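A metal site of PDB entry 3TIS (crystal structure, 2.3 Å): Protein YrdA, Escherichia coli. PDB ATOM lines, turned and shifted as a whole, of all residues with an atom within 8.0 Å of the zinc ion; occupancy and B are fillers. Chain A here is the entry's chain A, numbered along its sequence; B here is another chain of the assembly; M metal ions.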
ATOM      1  N   ARG A  45     -23.492  -6.029 -19.751  1.00  0.00           N
ATOM      2  CA  ARG A  45     -22.176  -6.596 -19.546  1.00  0.00           C
ATOM      3  C   ARG A  45     -21.412  -5.968 -18.384  1.00  0.00           C
ATOM      4  O   ARG A  45     -20.975  -4.814 -18.449  1.00  0.00           O
ATOM      5  CB  ARG A  45     -21.364  -6.495 -20.851  1.00  0.00           C
ATOM      6  CG  ARG A  45     -19.996  -7.194 -20.835  1.00  0.00           C
ATOM      7  CD  ARG A  45     -19.686  -7.891 -22.177  1.00  0.00           C
ATOM      8  NE  ARG A  45     -19.474  -6.971 -23.305  1.00  0.00           N
ATOM      9  CZ  ARG A  45     -18.339  -6.317 -23.539  1.00  0.00           C
ATOM     10  NH1 ARG A  45     -17.300  -6.484 -22.727  1.00  0.00           N
ATOM     11  NH2 ARG A  45     -18.237  -5.519 -24.591  1.00  0.00           N
ATOM     12  N   ASP A  47     -18.358  -6.932 -16.896  1.00  0.00           N
ATOM     13  CA  ASP A  47     -17.115  -7.679 -16.850  1.00  0.00           C
ATOM     14  C   ASP A  47     -15.940  -6.960 -16.214  1.00  0.00           C
ATOM     15  O   ASP A  47     -15.420  -7.406 -15.195  1.00  0.00           O
ATOM     16  CB  ASP A  47     -16.750  -8.173 -18.257  1.00  0.00           C
ATOM     17  CG  ASP A  47     -16.849  -7.077 -19.325  1.00  0.00           C
ATOM     18  OD1 ASP A  47     -16.689  -7.427 -20.517  1.00  0.00           O
ATOM     19  OD2 ASP A  47     -17.067  -5.890 -18.995  1.00  0.00           O
ATOM     20  N   VAL A  48     -15.506  -5.840 -16.783  1.00  0.00           N
ATOM     21  CA  VAL A  48     -14.387  -5.102 -16.213  1.00  0.00           C
ATOM     22  C   VAL A  48     -14.816  -4.305 -14.985  1.00  0.00           C
ATOM     23  O   VAL A  48     -13.990  -3.742 -14.274  1.00  0.00           O
ATOM     24  CB  VAL A  48     -13.720  -4.166 -17.243  1.00  0.00           C
ATOM     25  CG1 VAL A  48     -13.204  -4.985 -18.432  1.00  0.00           C
ATOM     26  CG2 VAL A  48     -14.699  -3.100 -17.719  1.00  0.00           C
ATOM     27  N   MET A  64     -28.708  -1.416 -24.361  1.00  0.00           N
ATOM     28  CA  MET A  64     -27.344  -1.878 -24.262  1.00  0.00           C
ATOM     29  C   MET A  64     -26.713  -1.223 -23.037  1.00  0.00           C
ATOM     30  O   MET A  64     -26.544  -0.005 -22.993  1.00  0.00           O
ATOM     31  CB  MET A  64     -26.604  -1.480 -25.540  1.00  0.00           C
ATOM     32  CG  MET A  64     -25.393  -2.303 -25.876  1.00  0.00           C
ATOM     33  SD  MET A  64     -24.054  -2.012 -24.736  1.00  0.00           S
ATOM     34  CE  MET A  64     -23.915  -3.630 -23.943  1.00  0.00           C
ATOM     35  N   LEU A  65     -26.373  -2.032 -22.040  1.00  0.00           N
ATOM     36  CA  LEU A  65     -25.783  -1.516 -20.799  1.00  0.00           C
ATOM     37  C   LEU A  65     -24.365  -2.030 -20.591  1.00  0.00           C
ATOM     38  O   LEU A  65     -24.148  -3.237 -20.560  1.00  0.00           O
ATOM     39  CB  LEU A  65     -26.619  -1.915 -19.576  1.00  0.00           C
ATOM     40  CG  LEU A  65     -27.957  -1.226 -19.297  1.00  0.00           C
ATOM     41  CD1 LEU A  65     -28.864  -1.250 -20.530  1.00  0.00           C
ATOM     42  CD2 LEU A  65     -28.612  -1.936 -18.133  1.00  0.00           C
ATOM     43  N   HIS A  66     -23.419  -1.113 -20.444  1.00  0.00           N
ATOM     44  CA  HIS A  66     -22.038  -1.501 -20.208  1.00  0.00           C
ATOM     45  C   HIS A  66     -21.323  -0.544 -19.254  1.00  0.00           C
ATOM     46  O   HIS A  66     -21.849   0.517 -18.913  1.00  0.00           O
ATOM     47  CB  HIS A  66     -21.266  -1.585 -21.525  1.00  0.00           C
ATOM     48  CG  HIS A  66     -19.997  -2.373 -21.418  1.00  0.00           C
ATOM     49  ND1 HIS A  66     -18.927  -2.202 -22.279  1.00  0.00           N
ATOM     50  CD2 HIS A  66     -19.617  -3.345 -20.554  1.00  0.00           C
ATOM     51  CE1 HIS A  66     -17.956  -3.028 -21.945  1.00  0.00           C
ATOM     52  NE2 HIS A  66     -18.346  -3.733 -20.902  1.00  0.00           N
ATOM     53  N   VAL A  67     -20.131  -0.935 -18.830  1.00  0.00           N
ATOM     54  CA  VAL A  67     -19.317  -0.155 -17.915  1.00  0.00           C
ATOM     55  C   VAL A  67     -18.124   0.468 -18.635  1.00  0.00           C
ATOM     56  O   VAL A  67     -17.804   0.110 -19.774  1.00  0.00           O
ATOM     57  CB  VAL A  67     -18.777  -1.036 -16.766  1.00  0.00           C
ATOM     58  CG1 VAL A  67     -19.941  -1.718 -16.041  1.00  0.00           C
ATOM     59  CG2 VAL A  67     -17.820  -2.071 -17.312  1.00  0.00           C
ATOM     60  N   THR A  68     -17.466   1.406 -17.967  1.00  0.00           N
ATOM     61  CA  THR A  68     -16.313   2.072 -18.549  1.00  0.00           C
ATOM     62  C   THR A  68     -15.143   1.124 -18.783  1.00  0.00           C
ATOM     63  O   THR A  68     -14.847   0.265 -17.959  1.00  0.00           O
ATOM     64  CB  THR A  68     -15.832   3.235 -17.669  1.00  0.00           C
ATOM     65  OG1 THR A  68     -16.828   4.269 -17.670  1.00  0.00           O
ATOM     66  CG2 THR A  68     -14.525   3.793 -18.187  1.00  0.00           C
ATOM     67  N   HIS A  69     -14.496   1.288 -19.932  1.00  0.00           N
ATOM     68  CA  HIS A  69     -13.359   0.475 -20.322  1.00  0.00           C
ATOM     69  C   HIS A  69     -12.102   0.902 -19.570  1.00  0.00           C
ATOM     70  O   HIS A  69     -11.964   2.068 -19.169  1.00  0.00           O
ATOM     71  CB  HIS A  69     -13.099   0.622 -21.828  1.00  0.00           C
ATOM     72  CG  HIS A  69     -14.280   0.270 -22.687  1.00  0.00           C
ATOM     73  ND1 HIS A  69     -14.250   0.383 -24.067  1.00  0.00           N
ATOM     74  CD2 HIS A  69     -15.508  -0.199 -22.373  1.00  0.00           C
ATOM     75  CE1 HIS A  69     -15.410  -0.008 -24.558  1.00  0.00           C
ATOM     76  NE2 HIS A  69     -16.184  -0.372 -23.556  1.00  0.00           N
ATOM     77  N   MET A  93     -28.804   3.318 -24.664  1.00  0.00           N
ATOM     78  CA  MET A  93     -27.437   2.901 -24.420  1.00  0.00           C
ATOM     79  C   MET A  93     -26.912   3.562 -23.149  1.00  0.00           C
ATOM     80  O   MET A  93     -26.883   4.787 -23.045  1.00  0.00           O
ATOM     81  CB  MET A  93     -26.551   3.267 -25.603  1.00  0.00           C
ATOM     82  CG  MET A  93     -25.127   2.796 -25.447  1.00  0.00           C
ATOM     83  SD  MET A  93     -24.360   2.454 -27.025  1.00  0.00           S
ATOM     84  CE  MET A  93     -24.892   0.779 -27.268  1.00  0.00           C
ATOM     85  N   LEU A  94     -26.526   2.740 -22.180  1.00  0.00           N
ATOM     86  CA  LEU A  94     -26.011   3.228 -20.913  1.00  0.00           C
ATOM     87  C   LEU A  94     -24.562   2.747 -20.811  1.00  0.00           C
ATOM     88  O   LEU A  94     -24.286   1.569 -20.978  1.00  0.00           O
ATOM     89  CB  LEU A  94     -26.840   2.685 -19.761  1.00  0.00           C
ATOM     90  CG  LEU A  94     -28.317   3.088 -19.772  1.00  0.00           C
ATOM     91  CD1 LEU A  94     -29.003   2.541 -18.543  1.00  0.00           C
ATOM     92  CD2 LEU A  94     -28.423   4.604 -19.796  1.00  0.00           C
ATOM     93  N   HIS A  95     -23.646   3.668 -20.514  1.00  0.00           N
ATOM     94  CA  HIS A  95     -22.246   3.302 -20.452  1.00  0.00           C
ATOM     95  C   HIS A  95     -21.449   3.928 -19.303  1.00  0.00           C
ATOM     96  O   HIS A  95     -21.107   5.106 -19.341  1.00  0.00           O
ATOM     97  CB  HIS A  95     -21.620   3.675 -21.808  1.00  0.00           C
ATOM     98  CG  HIS A  95     -20.350   2.951 -22.105  1.00  0.00           C
ATOM     99  ND1 HIS A  95     -19.135   3.337 -21.587  1.00  0.00           N
ATOM    100  CD2 HIS A  95     -20.115   1.840 -22.830  1.00  0.00           C
ATOM    101  CE1 HIS A  95     -18.205   2.481 -21.969  1.00  0.00           C
ATOM    102  NE2 HIS A  95     -18.772   1.559 -22.736  1.00  0.00           N
ATOM    103  N   GLY A  96     -21.142   3.131 -18.295  1.00  0.00           N
ATOM    104  CA  GLY A  96     -20.377   3.622 -17.161  1.00  0.00           C
ATOM    105  C   GLY A  96     -20.931   4.892 -16.538  1.00  0.00           C
ATOM    106  O   GLY A  96     -20.172   5.761 -16.109  1.00  0.00           O
ATOM    107  N   ASP A 113     -20.016   7.706 -20.413  1.00  0.00           N
ATOM    108  CA  ASP A 113     -19.198   7.518 -19.222  1.00  0.00           C
ATOM    109  C   ASP A 113     -19.151   8.688 -18.245  1.00  0.00           C
ATOM    110  O   ASP A 113     -18.957   9.844 -18.631  1.00  0.00           O
ATOM    111  CB  ASP A 113     -17.757   7.165 -19.629  1.00  0.00           C
ATOM    112  CG  ASP A 113     -17.710   6.018 -20.605  1.00  0.00           C
ATOM    113  OD1 ASP A 113     -17.985   6.235 -21.810  1.00  0.00           O
ATOM    114  OD2 ASP A 113     -17.398   4.882 -20.159  1.00  0.00           O
ATOM    115  N   GLN B  60     -18.280  -4.276 -31.289  1.00  0.00           N
ATOM    116  CA  GLN B  60     -18.935  -4.314 -29.993  1.00  0.00           C
ATOM    117  C   GLN B  60     -20.441  -4.575 -29.971  1.00  0.00           C
ATOM    118  O   GLN B  60     -21.135  -4.435 -30.979  1.00  0.00           O
ATOM    119  CB  GLN B  60     -18.595  -3.033 -29.232  1.00  0.00           C
ATOM    120  CG  GLN B  60     -17.094  -2.900 -28.990  1.00  0.00           C
ATOM    121  CD  GLN B  60     -16.729  -1.722 -28.122  1.00  0.00           C
ATOM    122  OE1 GLN B  60     -17.257  -1.556 -27.015  1.00  0.00           O
ATOM    123  NE2 GLN B  60     -15.807  -0.900 -28.595  1.00  0.00           N
ATOM    124  N   ASP B  61     -20.925  -4.953 -28.785  1.00  0.00           N
ATOM    125  CA  ASP B  61     -22.332  -5.293 -28.520  1.00  0.00           C
ATOM    126  C   ASP B  61     -23.381  -4.439 -29.224  1.00  0.00           C
ATOM    127  O   ASP B  61     -23.343  -3.219 -29.150  1.00  0.00           O
ATOM    128  CB  ASP B  61     -22.619  -5.218 -27.018  1.00  0.00           C
ATOM    129  CG  ASP B  61     -21.551  -5.876 -26.184  1.00  0.00           C
ATOM    130  OD1 ASP B  61     -20.378  -5.451 -26.269  1.00  0.00           O
ATOM    131  OD2 ASP B  61     -21.871  -6.820 -25.425  1.00  0.00           O
ATOM    132  N   GLY B  89     -17.599   0.771 -32.003  1.00  0.00           N
ATOM    133  CA  GLY B  89     -18.349   0.943 -30.770  1.00  0.00           C
ATOM    134  C   GLY B  89     -19.662   0.180 -30.681  1.00  0.00           C
ATOM    135  O   GLY B  89     -20.141  -0.391 -31.663  1.00  0.00           O
ATOM    136  N   HIS B  90     -20.255   0.197 -29.486  1.00  0.00           N
ATOM    137  CA  HIS B  90     -21.523  -0.467 -29.234  1.00  0.00           C
ATOM    138  C   HIS B  90     -22.630   0.128 -30.086  1.00  0.00           C
ATOM    139  O   HIS B  90     -22.628   1.326 -30.380  1.00  0.00           O
ATOM    140  CB  HIS B  90     -21.937  -0.298 -27.761  1.00  0.00           C
ATOM    141  CG  HIS B  90     -21.023  -0.945 -26.778  1.00  0.00           C
ATOM    142  ND1 HIS B  90     -20.855  -2.317 -26.695  1.00  0.00           N
ATOM    143  CD2 HIS B  90     -20.250  -0.420 -25.804  1.00  0.00           C
ATOM    144  CE1 HIS B  90     -20.025  -2.601 -25.716  1.00  0.00           C
ATOM    145  NE2 HIS B  90     -19.642  -1.463 -25.150  1.00  0.00           N
ATOM    146  N   MET B 107     -19.685   4.664 -30.190  1.00  0.00           N
ATOM    147  CA  MET B 107     -20.906   3.903 -29.987  1.00  0.00           C
ATOM    148  C   MET B 107     -22.135   4.710 -30.403  1.00  0.00           C
ATOM    149  O   MET B 107     -22.199   5.933 -30.180  1.00  0.00           O
ATOM    150  CB  MET B 107     -21.020   3.502 -28.499  1.00  0.00           C
ATOM    151  CG  MET B 107     -21.184   4.666 -27.534  1.00  0.00           C
ATOM    152  SD  MET B 107     -21.162   4.138 -25.793  1.00  0.00           S
ATOM    153  CE  MET B 107     -19.428   4.289 -25.414  1.00  0.00           C
ATOM    154  N   TYR B 167      -8.959  -4.532 -26.674  1.00  0.00           N
ATOM    155  CA  TYR B 167     -10.072  -5.407 -27.032  1.00  0.00           C
ATOM    156  C   TYR B 167      -9.618  -6.779 -27.524  1.00  0.00           C
ATOM    157  O   TYR B 167     -10.373  -7.744 -27.442  1.00  0.00           O
ATOM    158  CB  TYR B 167     -10.988  -4.738 -28.069  1.00  0.00           C
ATOM    159  CG  TYR B 167     -12.314  -4.320 -27.469  1.00  0.00           C
ATOM    160  CD1 TYR B 167     -12.524  -3.010 -27.016  1.00  0.00           C
ATOM    161  CD2 TYR B 167     -13.337  -5.251 -27.272  1.00  0.00           C
ATOM    162  CE1 TYR B 167     -13.731  -2.644 -26.383  1.00  0.00           C
ATOM    163  CE2 TYR B 167     -14.537  -4.896 -26.646  1.00  0.00           C
ATOM    164  CZ  TYR B 167     -14.727  -3.608 -26.201  1.00  0.00           C
ATOM    165  OH  TYR B 167     -15.899  -3.293 -25.573  1.00  0.00           O
ATOM    166  N   TRP B 170      -9.052  -8.538 -24.430  1.00  0.00           N
ATOM    167  CA  TRP B 170     -10.392  -8.665 -23.878  1.00  0.00           C
ATOM    168  C   TRP B 170     -11.125  -9.886 -24.470  1.00  0.00           C
ATOM    169  O   TRP B 170     -11.751 -10.649 -23.746  1.00  0.00           O
ATOM    170  CB  TRP B 170     -11.174  -7.394 -24.184  1.00  0.00           C
ATOM    171  CG  TRP B 170     -12.275  -7.094 -23.231  1.00  0.00           C
ATOM    172  CD1 TRP B 170     -13.061  -7.979 -22.553  1.00  0.00           C
ATOM    173  CD2 TRP B 170     -12.763  -5.788 -22.889  1.00  0.00           C
ATOM    174  NE1 TRP B 170     -14.018  -7.309 -21.828  1.00  0.00           N
ATOM    175  CE2 TRP B 170     -13.861  -5.959 -22.023  1.00  0.00           C
ATOM    176  CE3 TRP B 170     -12.384  -4.483 -23.254  1.00  0.00           C
ATOM    177  CZ2 TRP B 170     -14.577  -4.881 -21.499  1.00  0.00           C
ATOM    178  CZ3 TRP B 170     -13.109  -3.406 -22.735  1.00  0.00           C
ATOM    179  CH2 TRP B 170     -14.192  -3.616 -21.865  1.00  0.00           C
HETATM  180 ZN    ZN M   1     -18.444  -0.467 -23.538  1.00  0.00          ZN
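The zinc ion is bound by a ring nitrogen (ND1) of His 66.
The zinc ion is bound by a ring nitrogen (NE2) of His 95, 2.2 Å away.
A ring nitrogen (NE2) of His 90 of chain B binds the zinc ion, 2.2 Å away.
NE2 of His 69 binds the zinc ion, 2.3 Å away.
Residues that only touch the zinc ion: Gln 60 of chain B (3.8 Å) and Val 67 (3.9 Å).
Along chain A the residues within 4 Å of the zinc ion span positions 66 to 95.
The nearest printed residue that does not touch the zinc ion is Tyr 167 of chain B (4.3 Å).
O of His 66 sits at hydrogen-bond distance from N of Gly 96, 2.8 Å away.
The backbone carbonyl oxygen (O) of Leu 94 lies within hydrogen-bond range of the backbone NH (N) of His 66, 2.9 Å away.
A ring nitrogen (NE2) of His 66 is in hydrogen-bond range of the guanidinium group (NH1) of Arg 45.
The side-chain amide oxygen (OE1) of Gln 60 of chain B sits close to a ring nitrogen (NE2) of His 90 of chain B.
NE2 of His 95 sits close to O of Val 67, at 3.4 Å.
OE1 of Gln 60 of chain B sits at hydrogen-bond distance from OH of Tyr 167 of chain B (2.6 Å).
ND1 of His 95 sits at hydrogen-bond distance from OD2 of Asp 113.
SD of Met 64 is in hydrogen-bond range of ND1 of His 90 of chain B (3.8 Å).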
